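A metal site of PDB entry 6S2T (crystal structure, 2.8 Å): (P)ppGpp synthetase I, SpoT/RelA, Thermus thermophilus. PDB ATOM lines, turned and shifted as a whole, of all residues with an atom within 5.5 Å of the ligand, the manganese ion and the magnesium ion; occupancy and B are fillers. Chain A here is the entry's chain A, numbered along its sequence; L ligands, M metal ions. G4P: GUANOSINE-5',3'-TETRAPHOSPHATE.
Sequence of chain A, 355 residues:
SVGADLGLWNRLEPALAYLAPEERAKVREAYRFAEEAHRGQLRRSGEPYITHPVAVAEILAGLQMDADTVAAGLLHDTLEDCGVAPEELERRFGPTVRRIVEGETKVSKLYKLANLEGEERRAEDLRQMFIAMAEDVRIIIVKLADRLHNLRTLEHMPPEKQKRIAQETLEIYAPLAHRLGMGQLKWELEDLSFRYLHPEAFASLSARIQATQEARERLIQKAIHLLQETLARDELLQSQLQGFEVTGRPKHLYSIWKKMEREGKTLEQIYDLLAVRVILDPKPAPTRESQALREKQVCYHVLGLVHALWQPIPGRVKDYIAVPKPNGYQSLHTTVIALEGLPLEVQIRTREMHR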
ATOM      1  N   ARG A  43       6.270  26.731 -39.050  1.00  0.00           N
ATOM      2  CA  ARG A  43       5.239  26.236 -38.155  1.00  0.00           C
ATOM      3  C   ARG A  43       4.583  25.043 -38.877  1.00  0.00           C
ATOM      4  O   ARG A  43       4.738  24.905 -40.096  1.00  0.00           O
ATOM      5  CB  ARG A  43       4.197  27.337 -37.844  1.00  0.00           C
ATOM      6  CG  ARG A  43       4.695  28.441 -36.912  1.00  0.00           C
ATOM      7  CD  ARG A  43       4.488  28.131 -35.437  1.00  0.00           C
ATOM      8  NE  ARG A  43       3.163  28.526 -34.953  1.00  0.00           N
ATOM      9  CZ  ARG A  43       2.734  28.377 -33.698  1.00  0.00           C
ATOM     10  NH1 ARG A  43       3.549  27.869 -32.779  1.00  0.00           N
ATOM     11  NH2 ARG A  43       1.528  28.767 -33.351  1.00  0.00           N
ATOM     12  N   ARG A  44       3.838  24.196 -38.121  1.00  0.00           N
ATOM     13  CA  ARG A  44       3.088  23.054 -38.656  1.00  0.00           C
ATOM     14  C   ARG A  44       1.895  23.578 -39.477  1.00  0.00           C
ATOM     15  O   ARG A  44       0.985  22.821 -39.808  1.00  0.00           O
ATOM     16  CB  ARG A  44       2.620  22.104 -37.531  1.00  0.00           C
ATOM     17  CG  ARG A  44       3.685  21.144 -37.012  1.00  0.00           C
ATOM     18  CD  ARG A  44       3.150  20.302 -35.845  1.00  0.00           C
ATOM     19  NE  ARG A  44       2.891  18.909 -36.216  1.00  0.00           N
ATOM     20  CZ  ARG A  44       1.752  18.455 -36.759  1.00  0.00           C
ATOM     21  NH1 ARG A  44       0.755  19.289 -37.021  1.00  0.00           N
ATOM     22  NH2 ARG A  44       1.622  17.167 -37.048  1.00  0.00           N
ATOM     23  N   SER A  45       1.920  24.889 -39.797  1.00  0.00           N
ATOM     24  CA  SER A  45       0.931  25.624 -40.587  1.00  0.00           C
ATOM     25  C   SER A  45       1.528  26.001 -41.942  1.00  0.00           C
ATOM     26  O   SER A  45       0.782  26.387 -42.845  1.00  0.00           O
ATOM     27  CB  SER A  45       0.506  26.902 -39.856  1.00  0.00           C
ATOM     28  OG  SER A  45       1.536  27.878 -39.884  1.00  0.00           O
ATOM     29  N   TYR A  49       8.233  30.478 -38.595  1.00  0.00           N
ATOM     30  CA  TYR A  49       8.063  30.419 -37.147  1.00  0.00           C
ATOM     31  C   TYR A  49       7.835  31.785 -36.487  1.00  0.00           C
ATOM     32  O   TYR A  49       6.966  31.888 -35.621  1.00  0.00           O
ATOM     33  CB  TYR A  49       9.195  29.661 -36.437  1.00  0.00           C
ATOM     34  CG  TYR A  49       8.743  29.120 -35.096  1.00  0.00           C
ATOM     35  CD1 TYR A  49       8.085  27.895 -34.998  1.00  0.00           C
ATOM     36  CD2 TYR A  49       8.914  29.870 -33.931  1.00  0.00           C
ATOM     37  CE1 TYR A  49       7.638  27.417 -33.767  1.00  0.00           C
ATOM     38  CE2 TYR A  49       8.460  29.398 -32.697  1.00  0.00           C
ATOM     39  CZ  TYR A  49       7.822  28.175 -32.621  1.00  0.00           C
ATOM     40  OH  TYR A  49       7.376  27.711 -31.415  1.00  0.00           O
ATOM     41  N   HIS A  52       4.466  33.186 -34.888  1.00  0.00           N
ATOM     42  CA  HIS A  52       4.026  32.810 -33.543  1.00  0.00           C
ATOM     43  C   HIS A  52       4.563  33.778 -32.449  1.00  0.00           C
ATOM     44  O   HIS A  52       3.715  34.355 -31.777  1.00  0.00           O
ATOM     45  CB  HIS A  52       4.350  31.339 -33.224  1.00  0.00           C
ATOM     46  CG  HIS A  52       4.226  30.958 -31.770  1.00  0.00           C
ATOM     47  ND1 HIS A  52       3.002  30.818 -31.146  1.00  0.00           N
ATOM     48  CD2 HIS A  52       5.202  30.635 -30.885  1.00  0.00           C
ATOM     49  CE1 HIS A  52       3.266  30.441 -29.900  1.00  0.00           C
ATOM     50  NE2 HIS A  52       4.575  30.317 -29.702  1.00  0.00           N
ATOM     51  N   HIS A  76      10.315  34.102 -26.245  1.00  0.00           N
ATOM     52  CA  HIS A  76       9.922  32.956 -25.415  1.00  0.00           C
ATOM     53  C   HIS A  76      10.261  31.573 -25.998  1.00  0.00           C
ATOM     54  O   HIS A  76      10.164  30.594 -25.256  1.00  0.00           O
ATOM     55  CB  HIS A  76       8.420  33.021 -25.062  1.00  0.00           C
ATOM     56  CG  HIS A  76       7.512  32.615 -26.178  1.00  0.00           C
ATOM     57  ND1 HIS A  76       7.428  33.350 -27.343  1.00  0.00           N
ATOM     58  CD2 HIS A  76       6.682  31.557 -26.270  1.00  0.00           C
ATOM     59  CE1 HIS A  76       6.547  32.725 -28.103  1.00  0.00           C
ATOM     60  NE2 HIS A  76       6.085  31.625 -27.502  1.00  0.00           N
ATOM     61  N   ASP A  77      10.640  31.475 -27.290  1.00  0.00           N
ATOM     62  CA  ASP A  77      10.956  30.175 -27.900  1.00  0.00           C
ATOM     63  C   ASP A  77      12.392  30.072 -28.489  1.00  0.00           C
ATOM     64  O   ASP A  77      12.790  29.008 -28.978  1.00  0.00           O
ATOM     65  CB  ASP A  77       9.884  29.783 -28.958  1.00  0.00           C
ATOM     66  CG  ASP A  77       8.573  29.237 -28.374  1.00  0.00           C
ATOM     67  OD1 ASP A  77       8.637  28.397 -27.432  1.00  0.00           O
ATOM     68  OD2 ASP A  77       7.502  29.627 -28.874  1.00  0.00           O
ATOM     69  N   GLU A 104       8.944  30.576 -18.746  1.00  0.00           N
ATOM     70  CA  GLU A 104       7.910  30.069 -19.657  1.00  0.00           C
ATOM     71  C   GLU A 104       8.383  28.768 -20.333  1.00  0.00           C
ATOM     72  O   GLU A 104       7.576  27.866 -20.563  1.00  0.00           O
ATOM     73  CB  GLU A 104       7.533  31.134 -20.712  1.00  0.00           C
ATOM     74  CG  GLU A 104       6.330  30.796 -21.608  1.00  0.00           C
ATOM     75  CD  GLU A 104       6.573  30.061 -22.917  1.00  0.00           C
ATOM     76  OE1 GLU A 104       7.702  30.136 -23.459  1.00  0.00           O
ATOM     77  OE2 GLU A 104       5.615  29.418 -23.413  1.00  0.00           O
ATOM     78  N   SER A 108       6.727  24.411 -19.274  1.00  0.00           N
ATOM     79  CA  SER A 108       6.109  23.585 -20.331  1.00  0.00           C
ATOM     80  C   SER A 108       6.562  22.123 -20.213  1.00  0.00           C
ATOM     81  O   SER A 108       5.745  21.194 -20.321  1.00  0.00           O
ATOM     82  CB  SER A 108       6.429  24.149 -21.714  1.00  0.00           C
ATOM     83  OG  SER A 108       6.495  25.574 -21.789  1.00  0.00           O
ATOM     84  N   LYS A 143       3.020  32.596 -20.772  1.00  0.00           N
ATOM     85  CA  LYS A 143       2.596  31.226 -21.015  1.00  0.00           C
ATOM     86  C   LYS A 143       1.121  31.203 -21.467  1.00  0.00           C
ATOM     87  O   LYS A 143       0.762  30.439 -22.363  1.00  0.00           O
ATOM     88  CB  LYS A 143       2.815  30.348 -19.779  1.00  0.00           C
ATOM     89  CG  LYS A 143       2.441  28.869 -19.951  1.00  0.00           C
ATOM     90  CD  LYS A 143       3.453  28.035 -20.746  1.00  0.00           C
ATOM     91  CE  LYS A 143       2.890  27.481 -22.037  1.00  0.00           C
ATOM     92  NZ  LYS A 143       3.787  26.448 -22.591  1.00  0.00           N
ATOM     93  N   ASP A 146       0.910  32.517 -24.994  1.00  0.00           N
ATOM     94  CA  ASP A 146       1.480  31.478 -25.835  1.00  0.00           C
ATOM     95  C   ASP A 146       0.374  30.470 -26.130  1.00  0.00           C
ATOM     96  O   ASP A 146       0.073  30.233 -27.303  1.00  0.00           O
ATOM     97  CB  ASP A 146       2.707  30.835 -25.129  1.00  0.00           C
ATOM     98  CG  ASP A 146       3.289  29.587 -25.779  1.00  0.00           C
ATOM     99  OD1 ASP A 146       2.768  28.477 -25.512  1.00  0.00           O
ATOM    100  OD2 ASP A 146       4.282  29.718 -26.523  1.00  0.00           O
ATOM    101  N   ARG A 147      -0.265  29.914 -25.074  1.00  0.00           N
ATOM    102  CA  ARG A 147      -1.343  28.939 -25.203  1.00  0.00           C
ATOM    103  C   ARG A 147      -2.543  29.527 -25.955  1.00  0.00           C
ATOM    104  O   ARG A 147      -3.194  28.795 -26.700  1.00  0.00           O
ATOM    105  CB  ARG A 147      -1.736  28.354 -23.835  1.00  0.00           C
ATOM    106  CG  ARG A 147      -2.959  27.417 -23.827  1.00  0.00           C
ATOM    107  CD  ARG A 147      -2.781  26.164 -24.684  1.00  0.00           C
ATOM    108  NE  ARG A 147      -2.598  24.971 -23.856  1.00  0.00           N
ATOM    109  CZ  ARG A 147      -1.416  24.417 -23.614  1.00  0.00           C
ATOM    110  NH1 ARG A 147      -0.312  24.931 -24.137  1.00  0.00           N
ATOM    111  NH2 ARG A 147      -1.337  23.349 -22.850  1.00  0.00           N
ATOM    112  N   HIS A 149      -2.559  31.938 -28.550  1.00  0.00           N
ATOM    113  CA  HIS A 149      -2.183  31.888 -29.969  1.00  0.00           C
ATOM    114  C   HIS A 149      -2.084  30.455 -30.493  1.00  0.00           C
ATOM    115  O   HIS A 149      -2.462  30.205 -31.644  1.00  0.00           O
ATOM    116  CB  HIS A 149      -0.906  32.677 -30.263  1.00  0.00           C
ATOM    117  CG  HIS A 149      -0.460  32.563 -31.683  1.00  0.00           C
ATOM    118  ND1 HIS A 149       0.801  32.086 -32.021  1.00  0.00           N
ATOM    119  CD2 HIS A 149      -1.098  32.913 -32.830  1.00  0.00           C
ATOM    120  CE1 HIS A 149       0.882  32.152 -33.338  1.00  0.00           C
ATOM    121  NE2 HIS A 149      -0.238  32.644 -33.864  1.00  0.00           N
ATOM    122  N   ASN A 150      -1.597  29.540 -29.649  1.00  0.00           N
ATOM    123  CA  ASN A 150      -1.490  28.111 -29.959  1.00  0.00           C
ATOM    124  C   ASN A 150      -2.883  27.529 -30.293  1.00  0.00           C
ATOM    125  O   ASN A 150      -3.040  26.839 -31.309  1.00  0.00           O
ATOM    126  CB  ASN A 150      -0.854  27.370 -28.773  1.00  0.00           C
ATOM    127  CG  ASN A 150       0.573  26.910 -28.987  1.00  0.00           C
ATOM    128  OD1 ASN A 150       1.000  25.819 -28.546  1.00  0.00           O
ATOM    129  ND2 ASN A 150       1.337  27.745 -29.684  1.00  0.00           N
ATOM    130  N   LEU A 151      -3.887  27.860 -29.457  1.00  0.00           N
ATOM    131  CA  LEU A 151      -5.268  27.417 -29.623  1.00  0.00           C
ATOM    132  C   LEU A 151      -5.935  28.076 -30.832  1.00  0.00           C
ATOM    133  O   LEU A 151      -6.819  27.467 -31.452  1.00  0.00           O
ATOM    134  CB  LEU A 151      -6.085  27.729 -28.351  1.00  0.00           C
ATOM    135  CG  LEU A 151      -5.955  26.750 -27.184  1.00  0.00           C
ATOM    136  CD1 LEU A 151      -6.185  27.472 -25.881  1.00  0.00           C
ATOM    137  CD2 LEU A 151      -6.934  25.585 -27.310  1.00  0.00           C
ATOM    138  N   THR A 153      -4.537  28.727 -33.615  1.00  0.00           N
ATOM    139  CA  THR A 153      -3.952  28.005 -34.740  1.00  0.00           C
ATOM    140  C   THR A 153      -4.008  26.476 -34.536  1.00  0.00           C
ATOM    141  O   THR A 153      -3.166  25.758 -35.069  1.00  0.00           O
ATOM    142  CB  THR A 153      -2.501  28.478 -34.904  1.00  0.00           C
ATOM    143  OG1 THR A 153      -1.817  28.296 -33.667  1.00  0.00           O
ATOM    144  CG2 THR A 153      -2.404  29.937 -35.333  1.00  0.00           C
ATOM    145  N   LEU A 154      -4.990  25.962 -33.772  1.00  0.00           N
ATOM    146  CA  LEU A 154      -5.072  24.539 -33.468  1.00  0.00           C
ATOM    147  C   LEU A 154      -5.592  23.657 -34.634  1.00  0.00           C
ATOM    148  O   LEU A 154      -5.490  22.432 -34.552  1.00  0.00           O
ATOM    149  CB  LEU A 154      -5.888  24.319 -32.173  1.00  0.00           C
ATOM    150  CG  LEU A 154      -5.602  23.072 -31.330  1.00  0.00           C
ATOM    151  CD1 LEU A 154      -4.131  22.958 -30.948  1.00  0.00           C
ATOM    152  CD2 LEU A 154      -6.420  23.099 -30.073  1.00  0.00           C
ATOM    153  N   HIS A 156      -4.223  23.245 -37.526  1.00  0.00           N
ATOM    154  CA  HIS A 156      -3.024  22.651 -38.143  1.00  0.00           C
ATOM    155  C   HIS A 156      -2.419  21.526 -37.282  1.00  0.00           C
ATOM    156  O   HIS A 156      -1.260  21.141 -37.499  1.00  0.00           O
ATOM    157  CB  HIS A 156      -1.958  23.747 -38.418  1.00  0.00           C
ATOM    158  CG  HIS A 156      -2.528  24.941 -39.108  1.00  0.00           C
ATOM    159  ND1 HIS A 156      -2.774  26.107 -38.425  1.00  0.00           N
ATOM    160  CD2 HIS A 156      -2.940  25.076 -40.392  1.00  0.00           C
ATOM    161  CE1 HIS A 156      -3.302  26.941 -39.310  1.00  0.00           C
ATOM    162  NE2 HIS A 156      -3.417  26.359 -40.507  1.00  0.00           N
ATOM    163  N   MET A 157      -3.204  21.006 -36.318  1.00  0.00           N
ATOM    164  CA  MET A 157      -2.805  19.956 -35.392  1.00  0.00           C
ATOM    165  C   MET A 157      -3.725  18.733 -35.467  1.00  0.00           C
ATOM    166  O   MET A 157      -4.903  18.889 -35.788  1.00  0.00           O
ATOM    167  CB  MET A 157      -2.740  20.487 -33.932  1.00  0.00           C
ATOM    168  CG  MET A 157      -1.785  21.651 -33.734  1.00  0.00           C
ATOM    169  SD  MET A 157      -0.114  21.357 -34.341  1.00  0.00           S
ATOM    170  CE  MET A 157       0.648  20.724 -32.876  1.00  0.00           C
ATOM    171  N   LYS A 161      -4.068  15.875 -30.497  1.00  0.00           N
ATOM    172  CA  LYS A 161      -3.456  17.063 -29.910  1.00  0.00           C
ATOM    173  C   LYS A 161      -4.505  18.141 -29.629  1.00  0.00           C
ATOM    174  O   LYS A 161      -4.452  18.780 -28.573  1.00  0.00           O
ATOM    175  CB  LYS A 161      -2.319  17.603 -30.799  1.00  0.00           C
ATOM    176  CG  LYS A 161      -1.073  16.724 -30.779  1.00  0.00           C
ATOM    177  CD  LYS A 161       0.077  17.331 -31.564  1.00  0.00           C
ATOM    178  CE  LYS A 161       1.178  16.328 -31.857  1.00  0.00           C
ATOM    179  NZ  LYS A 161       2.260  16.906 -32.694  1.00  0.00           N
ATOM    180  N   ARG A 164      -6.184  17.051 -26.473  1.00  0.00           N
ATOM    181  CA  ARG A 164      -5.226  17.071 -25.370  1.00  0.00           C
ATOM    182  C   ARG A 164      -5.006  18.505 -24.889  1.00  0.00           C
ATOM    183  O   ARG A 164      -5.116  18.746 -23.691  1.00  0.00           O
ATOM    184  CB  ARG A 164      -3.895  16.414 -25.782  1.00  0.00           C
ATOM    185  CG  ARG A 164      -2.987  16.004 -24.600  1.00  0.00           C
ATOM    186  CD  ARG A 164      -2.030  17.101 -24.123  1.00  0.00           C
ATOM    187  NE  ARG A 164      -0.931  17.353 -25.063  1.00  0.00           N
ATOM    188  CZ  ARG A 164       0.003  18.287 -24.907  1.00  0.00           C
ATOM    189  NH1 ARG A 164      -0.012  19.082 -23.846  1.00  0.00           N
ATOM    190  NH2 ARG A 164       0.958  18.433 -25.815  1.00  0.00           N
ATOM    191  N   ILE A 165      -4.730  19.447 -25.823  1.00  0.00           N
ATOM    192  CA  ILE A 165      -4.477  20.874 -25.556  1.00  0.00           C
ATOM    193  C   ILE A 165      -5.674  21.553 -24.922  1.00  0.00           C
ATOM    194  O   ILE A 165      -5.512  22.250 -23.909  1.00  0.00           O
ATOM    195  CB  ILE A 165      -3.955  21.606 -26.833  1.00  0.00           C
ATOM    196  CG1 ILE A 165      -2.568  21.104 -27.253  1.00  0.00           C
ATOM    197  CG2 ILE A 165      -3.983  23.140 -26.713  1.00  0.00           C
ATOM    198  CD1 ILE A 165      -1.405  21.206 -26.192  1.00  0.00           C
ATOM    199  N   GLU A 168      -6.241  20.418 -21.230  1.00  0.00           N
ATOM    200  CA  GLU A 168      -5.170  21.019 -20.427  1.00  0.00           C
ATOM    201  C   GLU A 168      -5.442  22.503 -20.142  1.00  0.00           C
ATOM    202  O   GLU A 168      -5.297  22.952 -19.010  1.00  0.00           O
ATOM    203  CB  GLU A 168      -3.811  20.836 -21.105  1.00  0.00           C
ATOM    204  CG  GLU A 168      -2.673  20.900 -20.108  1.00  0.00           C
ATOM    205  CD  GLU A 168      -1.288  20.977 -20.703  1.00  0.00           C
ATOM    206  OE1 GLU A 168      -1.156  20.793 -21.941  1.00  0.00           O
ATOM    207  OE2 GLU A 168      -0.324  21.212 -19.942  1.00  0.00           O
ATOM    208  N   TYR A 173      -4.592  26.412 -17.569  1.00  0.00           N
ATOM    209  CA  TYR A 173      -4.407  27.793 -17.998  1.00  0.00           C
ATOM    210  C   TYR A 173      -5.629  28.719 -17.884  1.00  0.00           C
ATOM    211  O   TYR A 173      -5.440  29.850 -17.445  1.00  0.00           O
ATOM    212  CB  TYR A 173      -3.802  27.836 -19.403  1.00  0.00           C
ATOM    213  CG  TYR A 173      -2.500  27.054 -19.456  1.00  0.00           C
ATOM    214  CD1 TYR A 173      -1.319  27.569 -18.917  1.00  0.00           C
ATOM    215  CD2 TYR A 173      -2.460  25.765 -19.991  1.00  0.00           C
ATOM    216  CE1 TYR A 173      -0.136  26.841 -18.929  1.00  0.00           C
ATOM    217  CE2 TYR A 173      -1.277  25.022 -20.002  1.00  0.00           C
ATOM    218  CZ  TYR A 173      -0.120  25.563 -19.474  1.00  0.00           C
ATOM    219  OH  TYR A 173       1.038  24.832 -19.471  1.00  0.00           O
HETATM  220  PB  G4P L   1       5.748  19.361 -28.227  1.00  0.00           P
HETATM  221  O1B G4P L   1       7.101  19.962 -28.217  1.00  0.00           O
HETATM  222  O2B G4P L   1       5.884  17.785 -28.579  1.00  0.00           O
HETATM  223  O3B G4P L   1       5.064  19.567 -26.782  1.00  0.00           O
HETATM  224  O3A G4P L   1       4.856  20.093 -29.348  1.00  0.00           O
HETATM  225  PA  G4P L   1       3.316  19.604 -29.213  1.00  0.00           P
HETATM  226  O1A G4P L   1       3.169  18.447 -28.257  1.00  0.00           O
HETATM  227  O2A G4P L   1       2.889  19.075 -30.663  1.00  0.00           O
HETATM  228  O5' G4P L   1       2.287  20.786 -28.766  1.00  0.00           O
HETATM  229  C5' G4P L   1       2.682  22.193 -28.797  1.00  0.00           C
HETATM  230  C4' G4P L   1       3.923  22.638 -29.588  1.00  0.00           C
HETATM  231  O4' G4P L   1       3.553  22.512 -30.994  1.00  0.00           O
HETATM  232  C3' G4P L   1       4.099  24.191 -29.366  1.00  0.00           C
HETATM  233  O3' G4P L   1       5.261  24.609 -28.590  1.00  0.00           O
HETATM  234  C2' G4P L   1       4.227  24.786 -30.780  1.00  0.00           C
HETATM  235  O2' G4P L   1       5.429  25.542 -30.925  1.00  0.00           O
HETATM  236  C1' G4P L   1       4.218  23.565 -31.718  1.00  0.00           C
HETATM  237  N9  G4P L   1       3.584  23.935 -32.984  1.00  0.00           N
HETATM  238  C8  G4P L   1       4.201  23.953 -34.199  1.00  0.00           C
HETATM  239  N7  G4P L   1       3.366  24.360 -35.112  1.00  0.00           N
HETATM  240  C5  G4P L   1       2.175  24.627 -34.557  1.00  0.00           C
HETATM  241  C6  G4P L   1       0.951  25.095 -35.069  1.00  0.00           C
HETATM  242  O6  G4P L   1       0.838  25.352 -36.255  1.00  0.00           O
HETATM  243  N1  G4P L   1      -0.091  25.259 -34.224  1.00  0.00           N
HETATM  244  C2  G4P L   1       0.046  24.965 -32.888  1.00  0.00           C
HETATM  245  N2  G4P L   1      -1.023  25.119 -32.050  1.00  0.00           N
HETATM  246  N3  G4P L   1       1.198  24.539 -32.396  1.00  0.00           N
HETATM  247  C4  G4P L   1       2.271  24.350 -33.188  1.00  0.00           C
HETATM  248  PC  G4P L   1       4.847  25.181 -27.104  1.00  0.00           P
HETATM  249  O1C G4P L   1       5.016  26.660 -27.104  1.00  0.00           O
HETATM  250  O2C G4P L   1       5.858  24.602 -25.981  1.00  0.00           O
HETATM  251  O3C G4P L   1       3.286  24.885 -26.763  1.00  0.00           O
HETATM  252  PD  G4P L   1       3.136  23.629 -25.741  1.00  0.00           P
HETATM  253  O1D G4P L   1       4.172  22.606 -26.007  1.00  0.00           O
HETATM  254  O2D G4P L   1       1.714  22.933 -25.971  1.00  0.00           O
HETATM  255  O3D G4P L   1       3.266  24.139 -24.226  1.00  0.00           O
HETATM  256 MN    MN M   1       5.510  28.901 -28.064  1.00  0.00          MN
HETATM  257 MG    MG M   2       1.363  26.490 -25.261  1.00  0.00          MG
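An oxygen (O2D) of the ligand lies close to the guanidinium group (NH1) of Arg 147 (3.4 Å).
O of Asn 150 is in hydrogen-bond range of N2 of the ligand, 2.8 Å away.
The side-chain amide oxygen (OD1) of Asn 150 lies close to an oxygen (O3C) of the ligand, at 3.0 Å.
O3D of the ligand is in salt-bridge range of NZ of Lys 143 (2.9 Å).
OH of Tyr 49 is in hydrogen-bond range of O2' of the ligand.
The side-chain amino group (NZ) of Lys 161 lies within salt-bridge range of an oxygen (O2A) of the ligand.
The backbone NH (N) of Arg 44 lies within hydrogen-bond range of a nitrogen (N7) of the ligand (3.1 Å).
O of Thr 153 lies within hydrogen-bond range of N1 of the ligand, at 3.2 Å.
An oxygen (O1A) of the ligand is in salt-bridge range of the guanidinium group (NH2) of Arg 164 (3.3 Å).
A ring nitrogen (NE2) of His 76 lies close to the side-chain carboxylate of Asp 146.
The side-chain carboxylate (OD1) of Asp 146 sits close to the side-chain amino group (NZ) of Lys 143.
OD2 of Asp 77 sits close to OH of Tyr 49 (3.2 Å).
ND1 of His 52 is in hydrogen-bond range of ND1 of His 149.
The side-chain amino group (NZ) of Lys 143 is in hydrogen-bond range of the side-chain hydroxyl (OG) of Ser 108.
The side-chain carboxylate (OE2) of Glu 104 is in salt-bridge range of the side-chain amino group (NZ) of Lys 143 (3.6 Å).
The side-chain hydroxyl (OG1) of Thr 153 is in hydrogen-bond range of the guanidinium group (NH2) of Arg 43.
NH1 of Arg 164 lies within salt-bridge range of OE1 of Glu 168 (2.8 Å).
Arg 43 touches the ligand (NH1 to O2', 3.5 Å).
Ser 45 touches the ligand.
Leu 154 touches the ligand (CD1 to N2, 3.9 Å).
CB of His 156 touches O6 of the ligand, at 3.9 Å.
Met 157 touches the ligand.
Ile 165 touches the ligand.
Hydrophobic or aromatic side chains within 4 Å of the ligand: Tyr 49, Leu 154, His 156, Met 157 and Ile 165.
Of the 24 residues printed, 15 come within 4 Å of the ligand.
Four residues have an atom within 4 Å of the manganese ion: His 52, His 76, Asp 77 and Asp 146.
Merely in contact with the magnesium ion: Lys 143 (3.6 Å) and Asn 150 (3.4 Å).
Four residues have an atom within 4 Å of the magnesium ion: Lys 143, Asp 146, Arg 147 and Asn 150.
The nearest printed residue that does not touch the magnesium ion is Glu 104 (5.5 Å).
The manganese ion is bound by the side-chain carboxylate of Asp 146 (2.1 Å), the side-chain carboxylate of Asp 77 (2.3 Å), a ring nitrogen (NE2) of His 52 (2.4 Å) and an oxygen (O1C) of the ligand (2.5 Å).
Slightly farther from the manganese ion lies a ring nitrogen (NE2) of His 76 (2.8 Å).
OD1 of Asp 146 is bound to the magnesium ion (2.4 Å).
The guanidinium group (NH1) of Arg 147 binds the magnesium ion.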
